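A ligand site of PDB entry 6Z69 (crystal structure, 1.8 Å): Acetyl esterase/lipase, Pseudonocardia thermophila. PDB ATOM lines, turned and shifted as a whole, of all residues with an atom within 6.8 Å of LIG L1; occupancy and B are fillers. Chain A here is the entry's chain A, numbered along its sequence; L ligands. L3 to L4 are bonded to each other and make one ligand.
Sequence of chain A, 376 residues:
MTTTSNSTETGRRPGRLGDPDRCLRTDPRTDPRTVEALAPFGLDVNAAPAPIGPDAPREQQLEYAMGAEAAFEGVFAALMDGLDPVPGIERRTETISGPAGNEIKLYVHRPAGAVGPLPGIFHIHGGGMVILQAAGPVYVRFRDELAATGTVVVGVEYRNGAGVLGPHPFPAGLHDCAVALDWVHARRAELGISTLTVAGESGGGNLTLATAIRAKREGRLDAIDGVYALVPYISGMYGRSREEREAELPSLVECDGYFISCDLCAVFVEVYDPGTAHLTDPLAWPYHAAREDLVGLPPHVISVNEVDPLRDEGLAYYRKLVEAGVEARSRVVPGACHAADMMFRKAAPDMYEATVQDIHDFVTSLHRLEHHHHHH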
ATOM      1  N   LEU A  43     -15.609   9.953  -3.632  1.00  0.00           N
ATOM      2  CA  LEU A  43     -15.576   8.844  -2.629  1.00  0.00           C
ATOM      3  C   LEU A  43     -16.954   8.604  -2.012  1.00  0.00           C
ATOM      4  O   LEU A  43     -17.030   7.832  -1.032  1.00  0.00           O
ATOM      5  CB  LEU A  43     -14.546   9.152  -1.549  1.00  0.00           C
ATOM      6  CG  LEU A  43     -13.093   9.139  -2.022  1.00  0.00           C
ATOM      7  CD1 LEU A  43     -12.158   9.670  -0.970  1.00  0.00           C
ATOM      8  CD2 LEU A  43     -12.683   7.730  -2.431  1.00  0.00           C
ATOM      9  N   ALA A  47     -15.623   2.769  -5.528  1.00  0.00           N
ATOM     10  CA  ALA A  47     -14.467   2.782  -6.432  1.00  0.00           C
ATOM     11  C   ALA A  47     -14.623   1.634  -7.441  1.00  0.00           C
ATOM     12  O   ALA A  47     -15.173   0.556  -7.095  1.00  0.00           O
ATOM     13  CB  ALA A  47     -13.178   2.686  -5.658  1.00  0.00           C
ATOM     14  N   ALA A  68      -1.641   5.540  -4.227  1.00  0.00           N
ATOM     15  CA  ALA A  68      -2.798   5.576  -3.322  1.00  0.00           C
ATOM     16  C   ALA A  68      -2.446   6.468  -2.135  1.00  0.00           C
ATOM     17  O   ALA A  68      -3.274   7.276  -1.736  1.00  0.00           O
ATOM     18  CB  ALA A  68      -3.152   4.200  -2.849  1.00  0.00           C
ATOM     19  N   PHE A  72      -4.515   9.832  -1.214  1.00  0.00           N
ATOM     20  CA  PHE A  72      -5.235   9.865   0.090  1.00  0.00           C
ATOM     21  C   PHE A  72      -4.660  10.934   1.033  1.00  0.00           C
ATOM     22  O   PHE A  72      -5.442  11.583   1.733  1.00  0.00           O
ATOM     23  CB  PHE A  72      -5.290   8.467   0.707  1.00  0.00           C
ATOM     24  CG  PHE A  72      -6.494   7.726   0.168  1.00  0.00           C
ATOM     25  CD1 PHE A  72      -7.780   8.146   0.514  1.00  0.00           C
ATOM     26  CD2 PHE A  72      -6.353   6.715  -0.761  1.00  0.00           C
ATOM     27  CE1 PHE A  72      -8.898   7.505  -0.004  1.00  0.00           C
ATOM     28  CE2 PHE A  72      -7.480   6.065  -1.263  1.00  0.00           C
ATOM     29  CZ  PHE A  72      -8.751   6.468  -0.892  1.00  0.00           C
ATOM     30  N   PHE A  76      -6.963  13.818   2.694  1.00  0.00           N
ATOM     31  CA  PHE A  76      -6.895  14.080   4.159  1.00  0.00           C
ATOM     32  C   PHE A  76      -6.490  15.521   4.403  1.00  0.00           C
ATOM     33  O   PHE A  76      -7.114  16.176   5.283  1.00  0.00           O
ATOM     34  CB  PHE A  76      -5.982  13.061   4.833  1.00  0.00           C
ATOM     35  CG  PHE A  76      -6.516  11.655   4.728  1.00  0.00           C
ATOM     36  CD1 PHE A  76      -7.879  11.413   4.630  1.00  0.00           C
ATOM     37  CD2 PHE A  76      -5.656  10.589   4.643  1.00  0.00           C
ATOM     38  CE1 PHE A  76      -8.380  10.131   4.540  1.00  0.00           C
ATOM     39  CE2 PHE A  76      -6.152   9.305   4.503  1.00  0.00           C
ATOM     40  CZ  PHE A  76      -7.508   9.085   4.462  1.00  0.00           C
ATOM     41  N   GLY A 126      -3.372   4.853  11.263  1.00  0.00           N
ATOM     42  CA  GLY A 126      -3.841   3.914  10.239  1.00  0.00           C
ATOM     43  C   GLY A 126      -3.196   4.110   8.869  1.00  0.00           C
ATOM     44  O   GLY A 126      -2.239   4.927   8.708  1.00  0.00           O
ATOM     45  N   GLY A 127      -3.691   3.355   7.913  1.00  0.00           N
ATOM     46  CA  GLY A 127      -3.101   3.206   6.565  1.00  0.00           C
ATOM     47  C   GLY A 127      -2.711   1.774   6.300  1.00  0.00           C
ATOM     48  O   GLY A 127      -1.740   1.549   5.562  1.00  0.00           O
ATOM     49  N   GLY A 128      -3.448   0.816   6.854  1.00  0.00           N
ATOM     50  CA  GLY A 128      -3.289  -0.628   6.520  1.00  0.00           C
ATOM     51  C   GLY A 128      -1.902  -1.163   6.814  1.00  0.00           C
ATOM     52  O   GLY A 128      -1.529  -2.197   6.224  1.00  0.00           O
ATOM     53  N   MET A 129      -1.167  -0.526   7.740  1.00  0.00           N
ATOM     54  CA  MET A 129       0.250  -0.809   8.111  1.00  0.00           C
ATOM     55  C   MET A 129       1.187  -0.643   6.914  1.00  0.00           C
ATOM     56  O   MET A 129       2.395  -0.989   7.053  1.00  0.00           O
ATOM     57  CB  MET A 129       0.390  -2.208   8.702  1.00  0.00           C
ATOM     58  CG  MET A 129      -0.502  -2.417   9.912  1.00  0.00           C
ATOM     59  SD  MET A 129      -2.171  -3.072   9.589  1.00  0.00           S
ATOM     60  CE  MET A 129      -1.790  -4.696   8.940  1.00  0.00           C
ATOM     61  N   VAL A 130       0.682  -0.088   5.803  1.00  0.00           N
ATOM     62  CA  VAL A 130       1.460   0.043   4.541  1.00  0.00           C
ATOM     63  C   VAL A 130       1.633   1.506   4.089  1.00  0.00           C
ATOM     64  O   VAL A 130       2.631   1.758   3.415  1.00  0.00           O
ATOM     65  CB  VAL A 130       0.879  -0.843   3.428  1.00  0.00           C
ATOM     66  CG1 VAL A 130       0.995  -2.301   3.863  1.00  0.00           C
ATOM     67  CG2 VAL A 130      -0.542  -0.486   3.046  1.00  0.00           C
ATOM     68  N   ILE A 131       0.703   2.426   4.399  1.00  0.00           N
ATOM     69  CA  ILE A 131       0.797   3.805   3.861  1.00  0.00           C
ATOM     70  C   ILE A 131       0.366   4.829   4.936  1.00  0.00           C
ATOM     71  O   ILE A 131      -0.207   4.414   5.996  1.00  0.00           O
ATOM     72  CB  ILE A 131       0.006   3.996   2.554  1.00  0.00           C
ATOM     73  CG1 ILE A 131      -1.480   3.661   2.732  1.00  0.00           C
ATOM     74  CG2 ILE A 131       0.622   3.209   1.406  1.00  0.00           C
ATOM     75  CD1 ILE A 131      -2.336   4.146   1.587  1.00  0.00           C
ATOM     76  N   LEU A 132       0.653   6.118   4.634  1.00  0.00           N
ATOM     77  CA  LEU A 132       0.234   7.337   5.372  1.00  0.00           C
ATOM     78  C   LEU A 132       1.262   7.627   6.481  1.00  0.00           C
ATOM     79  O   LEU A 132       1.872   6.679   6.998  1.00  0.00           O
ATOM     80  CB  LEU A 132      -1.163   7.181   6.003  1.00  0.00           C
ATOM     81  CG  LEU A 132      -2.311   6.881   5.038  1.00  0.00           C
ATOM     82  CD1 LEU A 132      -3.642   6.729   5.817  1.00  0.00           C
ATOM     83  CD2 LEU A 132      -2.404   7.911   3.912  1.00  0.00           C
ATOM     84  N   SER A 202      -8.033   1.451  12.461  1.00  0.00           N
ATOM     85  CA  SER A 202      -7.877   0.700  11.183  1.00  0.00           C
ATOM     86  C   SER A 202      -6.561  -0.048  11.278  1.00  0.00           C
ATOM     87  O   SER A 202      -6.412  -0.776  12.251  1.00  0.00           O
ATOM     88  CB  SER A 202      -8.014   1.654  10.010  1.00  0.00           C
ATOM     89  OG  SER A 202      -8.102   0.969   8.767  1.00  0.00           O
ATOM     90  N   GLY A 203      -5.592   0.211  10.395  1.00  0.00           N
ATOM     91  CA  GLY A 203      -4.266  -0.432  10.507  1.00  0.00           C
ATOM     92  C   GLY A 203      -3.594  -0.125  11.842  1.00  0.00           C
ATOM     93  O   GLY A 203      -2.846  -0.953  12.331  1.00  0.00           O
ATOM     94  N   TYR A 233      -8.579  -3.042  11.682  1.00  0.00           N
ATOM     95  CA  TYR A 233      -8.288  -3.726  10.396  1.00  0.00           C
ATOM     96  C   TYR A 233      -7.507  -4.995  10.706  1.00  0.00           C
ATOM     97  O   TYR A 233      -6.269  -4.933  10.700  1.00  0.00           O
ATOM     98  CB  TYR A 233      -7.543  -2.730   9.514  1.00  0.00           C
ATOM     99  CG  TYR A 233      -6.980  -3.233   8.212  1.00  0.00           C
ATOM    100  CD1 TYR A 233      -7.780  -3.493   7.117  1.00  0.00           C
ATOM    101  CD2 TYR A 233      -5.599  -3.331   8.052  1.00  0.00           C
ATOM    102  CE1 TYR A 233      -7.242  -3.916   5.915  1.00  0.00           C
ATOM    103  CE2 TYR A 233      -5.050  -3.746   6.849  1.00  0.00           C
ATOM    104  CZ  TYR A 233      -5.860  -4.002   5.763  1.00  0.00           C
ATOM    105  OH  TYR A 233      -5.279  -4.384   4.585  1.00  0.00           O
ATOM    106  N   PHE A 259     -16.045   3.635   1.165  1.00  0.00           N
ATOM    107  CA  PHE A 259     -14.755   4.324   1.462  1.00  0.00           C
ATOM    108  C   PHE A 259     -13.559   3.382   1.209  1.00  0.00           C
ATOM    109  O   PHE A 259     -12.565   3.761   0.505  1.00  0.00           O
ATOM    110  CB  PHE A 259     -14.715   4.898   2.886  1.00  0.00           C
ATOM    111  CG  PHE A 259     -13.488   5.752   3.097  1.00  0.00           C
ATOM    112  CD1 PHE A 259     -13.367   6.965   2.450  1.00  0.00           C
ATOM    113  CD2 PHE A 259     -12.442   5.309   3.883  1.00  0.00           C
ATOM    114  CE1 PHE A 259     -12.217   7.734   2.590  1.00  0.00           C
ATOM    115  CE2 PHE A 259     -11.282   6.063   4.007  1.00  0.00           C
ATOM    116  CZ  PHE A 259     -11.176   7.262   3.368  1.00  0.00           C
ATOM    117  N   ILE A 260     -13.591   2.183   1.788  1.00  0.00           N
ATOM    118  CA  ILE A 260     -12.534   1.145   1.564  1.00  0.00           C
ATOM    119  C   ILE A 260     -13.114  -0.073   0.859  1.00  0.00           C
ATOM    120  O   ILE A 260     -14.346  -0.366   1.019  1.00  0.00           O
ATOM    121  CB  ILE A 260     -11.801   0.797   2.873  1.00  0.00           C
ATOM    122  CG1 ILE A 260     -12.734   0.248   3.947  1.00  0.00           C
ATOM    123  CG2 ILE A 260     -10.954   1.991   3.384  1.00  0.00           C
ATOM    124  CD1 ILE A 260     -11.991  -0.479   5.048  1.00  0.00           C
ATOM    125  N   SER A 261     -12.258  -0.758   0.090  1.00  0.00           N
ATOM    126  CA  SER A 261     -12.636  -1.889  -0.782  1.00  0.00           C
ATOM    127  C   SER A 261     -11.788  -3.088  -0.428  1.00  0.00           C
ATOM    128  O   SER A 261     -10.579  -2.973  -0.249  1.00  0.00           O
ATOM    129  CB  SER A 261     -12.579  -1.555  -2.247  1.00  0.00           C
ATOM    130  OG  SER A 261     -13.369  -0.398  -2.525  1.00  0.00           O
ATOM    131  N   CYS A 262     -12.442  -4.225  -0.313  1.00  0.00           N
ATOM    132  CA  CYS A 262     -11.778  -5.512  -0.044  1.00  0.00           C
ATOM    133  C   CYS A 262     -10.690  -5.806  -1.108  1.00  0.00           C
ATOM    134  O   CYS A 262      -9.658  -6.318  -0.716  1.00  0.00           O
ATOM    135  CB  CYS A 262     -12.765  -6.665   0.015  1.00  0.00           C
ATOM    136  SG  CYS A 262     -13.650  -6.731   1.594  1.00  0.00           S
ATOM    137  N   ASP A 263     -10.905  -5.500  -2.388  1.00  0.00           N
ATOM    138  CA  ASP A 263      -9.902  -5.821  -3.441  1.00  0.00           C
ATOM    139  C   ASP A 263      -8.589  -5.048  -3.173  1.00  0.00           C
ATOM    140  O   ASP A 263      -7.531  -5.680  -3.231  1.00  0.00           O
ATOM    141  CB  ASP A 263     -10.474  -5.700  -4.866  1.00  0.00           C
ATOM    142  CG  ASP A 263     -11.098  -4.365  -5.253  1.00  0.00           C
ATOM    143  OD1 ASP A 263     -11.015  -3.407  -4.455  1.00  0.00           O
ATOM    144  OD2 ASP A 263     -11.662  -4.294  -6.374  1.00  0.00           O
ATOM    145  N   LEU A 264      -8.650  -3.762  -2.886  1.00  0.00           N
ATOM    146  CA  LEU A 264      -7.412  -2.984  -2.608  1.00  0.00           C
ATOM    147  C   LEU A 264      -6.817  -3.464  -1.278  1.00  0.00           C
ATOM    148  O   LEU A 264      -5.603  -3.630  -1.225  1.00  0.00           O
ATOM    149  CB  LEU A 264      -7.706  -1.480  -2.610  1.00  0.00           C
ATOM    150  CG  LEU A 264      -6.464  -0.607  -2.457  1.00  0.00           C
ATOM    151  CD1 LEU A 264      -5.367  -1.072  -3.407  1.00  0.00           C
ATOM    152  CD2 LEU A 264      -6.796   0.854  -2.627  1.00  0.00           C
ATOM    153  N   CYS A 265      -7.639  -3.733  -0.257  1.00  0.00           N
ATOM    154  CA  CYS A 265      -7.106  -4.230   1.037  1.00  0.00           C
ATOM    155  C   CYS A 265      -6.390  -5.554   0.762  1.00  0.00           C
ATOM    156  O   CYS A 265      -5.326  -5.791   1.338  1.00  0.00           O
ATOM    157  CB  CYS A 265      -8.192  -4.386   2.083  1.00  0.00           C
ATOM    158  SG  CYS A 265      -8.870  -2.795   2.635  1.00  0.00           S
ATOM    159  N   PHE A 268      -3.077  -4.897  -0.184  1.00  0.00           N
ATOM    160  CA  PHE A 268      -2.283  -4.291   0.918  1.00  0.00           C
ATOM    161  C   PHE A 268      -1.895  -5.397   1.916  1.00  0.00           C
ATOM    162  O   PHE A 268      -0.860  -5.280   2.596  1.00  0.00           O
ATOM    163  CB  PHE A 268      -3.065  -3.145   1.574  1.00  0.00           C
ATOM    164  CG  PHE A 268      -3.118  -1.835   0.825  1.00  0.00           C
ATOM    165  CD1 PHE A 268      -2.419  -1.648  -0.361  1.00  0.00           C
ATOM    166  CD2 PHE A 268      -3.909  -0.808   1.299  1.00  0.00           C
ATOM    167  CE1 PHE A 268      -2.493  -0.441  -1.025  1.00  0.00           C
ATOM    168  CE2 PHE A 268      -3.971   0.408   0.633  1.00  0.00           C
ATOM    169  CZ  PHE A 268      -3.269   0.570  -0.539  1.00  0.00           C
HETATM  170  C1  LIG L   1      -8.476   3.693   0.998  1.00  0.00           C
HETATM  171  C2  LIG L   1      -9.243   2.825   0.204  1.00  0.00           C
HETATM  172  C3  LIG L   1      -9.054   1.391   0.316  1.00  0.00           C
HETATM  173  C4  LIG L   1      -5.653   2.035   3.648  1.00  0.00           C
HETATM  174  C5  LIG L   1      -5.764   3.517   3.613  1.00  0.00           C
HETATM  175  C6  LIG L   1      -6.701   4.016   2.744  1.00  0.00           C
HETATM  176  O1  LIG L   1      -4.767   1.449   4.499  1.00  0.00           O
HETATM  177  O2  LIG L   1      -6.446   1.217   2.894  1.00  0.00           O
HETATM  178  C7  LIG L   1      -6.844   5.527   2.693  1.00  0.00           C
HETATM  179  C8  LIG L   1      -7.484   3.189   1.924  1.00  0.00           C
HETATM  180  C9  LIG L   1      -7.362   1.734   2.009  1.00  0.00           C
HETATM  181  C10 LIG L   1      -8.100   0.881   1.268  1.00  0.00           C
HETATM  182  O3  LIG L   1      -9.848   0.567  -0.495  1.00  0.00           O
HETATM  183  C1  LG2 L   2      -7.942   2.873   6.792  1.00  0.00           C
HETATM  184  C2  LG2 L   2      -7.725   4.151   7.548  1.00  0.00           C
HETATM  185  C3  LG2 L   2      -8.073   5.355   6.699  1.00  0.00           C
HETATM  186  C4  LG2 L   2      -7.506   6.607   7.364  1.00  0.00           C
HETATM  187  C5  LG2 L   2      -8.284   7.033   8.605  1.00  0.00           C
HETATM  188  C6  LG2 L   2      -8.113   8.554   8.820  1.00  0.00           C
HETATM  189  P1  LG2 L   2      -7.291   1.428   7.577  1.00  0.00           P
HETATM  190  O1  LG2 L   2      -5.859   1.553   7.991  1.00  0.00           O
HETATM  191  O2  LG2 L   2      -7.571   0.489   6.301  1.00  0.00           O
HETATM  192  C7  LG2 L   2      -7.408  -0.828   6.335  1.00  0.00           C
HETATM  193  C1  LG3 L   3      -6.005   6.127  -5.870  1.00  0.00           C
HETATM  194  C2  LG3 L   3      -7.005   7.273  -5.756  1.00  0.00           C
HETATM  195  C3  LG3 L   3      -7.527   7.449  -4.323  1.00  0.00           C
HETATM  196  C4  LG3 L   3      -8.782   8.343  -4.228  1.00  0.00           C
HETATM  197  C5  LG3 L   3      -8.527   9.793  -4.677  1.00  0.00           C
HETATM  198  C6  LG3 L   3      -9.671  10.743  -4.388  1.00  0.00           C
HETATM  199  P1  LG3 L   3      -4.891   6.351  -7.345  1.00  0.00           P
HETATM  200  O1  LG3 L   3      -5.429   5.941  -8.660  1.00  0.00           O
HETATM  201  O2  LG3 L   3      -3.476   5.541  -7.002  1.00  0.00           O
HETATM  202  C7  LG3 L   3      -3.005   4.403  -7.673  1.00  0.00           C
HETATM  203  C1  LG4 L   4      -2.475   8.834 -10.342  1.00  0.00           C
HETATM  204  C2  LG4 L   4      -3.533   8.311  -9.579  1.00  0.00           C
HETATM  205  C3  LG4 L   4      -3.371   8.234  -8.154  1.00  0.00           C
HETATM  206  C4  LG4 L   4       0.949  10.017  -8.227  1.00  0.00           C
HETATM  207  C5  LG4 L   4       0.938  10.178  -9.719  1.00  0.00           C
HETATM  208  C6  LG4 L   4      -0.184   9.780 -10.383  1.00  0.00           C
HETATM  209  O1  LG4 L   4       2.040  10.371  -7.502  1.00  0.00           O
HETATM  210  O2  LG4 L   4      -0.090   9.518  -7.543  1.00  0.00           O
HETATM  211  C7  LG4 L   4      -0.210   9.922 -11.909  1.00  0.00           C
HETATM  212  C8  LG4 L   4      -1.247   9.277  -9.704  1.00  0.00           C
HETATM  213  C9  LG4 L   4      -1.191   9.155  -8.253  1.00  0.00           C
HETATM  214  C10 LG4 L   4      -2.185   8.685  -7.524  1.00  0.00           C
HETATM  215  O3  LG4 L   4      -4.378   7.744  -7.353  1.00  0.00           O
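The backbone NH (N) of Gly 128 lies within hydrogen-bond range of an oxygen (O1) of LIG L1.
An oxygen (O3) of LIG L1 is in hydrogen-bond range of the backbone NH (N) of Ser 261 (2.8 Å).
The backbone NH of Gly 127 is in hydrogen-bond range of an oxygen (O1) of LG2 L2 (2.8 Å).
The backbone NH (N) of Gly 128 sits at hydrogen-bond distance from an oxygen (O1) of LG2 L2 (2.8 Å).
OG of Ser 202 is covalently linked to P1 of LG2 L2.
The backbone NH of Gly 203 lies within hydrogen-bond range of an oxygen (O1) of LG2 L2, at 2.8 Å.
An oxygen (O2) of LG3 L3 sits at hydrogen-bond distance from the backbone NH (N) of Ala 68 (3.3 Å).
The side-chain sulfur of Cys 265 is in hydrogen-bond range of the backbone carbonyl oxygen of Ser 261 (3.4 Å).
O1 of LIG L1 lies close to O of Gly 127.
Phe 72 touches LIG L1 (CG to C7, 3.4 Å).
Phe 259 touches LIG L1.
Ile 260 touches LIG L1.
CB of Leu 264 touches O3 of LIG L1, at 3.6 Å.
SG of Cys 265 touches C10 of LIG L1, 3.997 Å away.
CE2 of Phe 268 touches O2 of LIG L1 (3.4 Å).
Nine residues have an atom within 4 Å of LIG L1: Phe 72, Gly 127, Gly 128, Phe 259, Ile 260, Ser 261, Leu 264, Cys 265 and Phe 268.
The nearest printed residue that does not touch LIG L1 is Phe 76 (4.03 Å).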
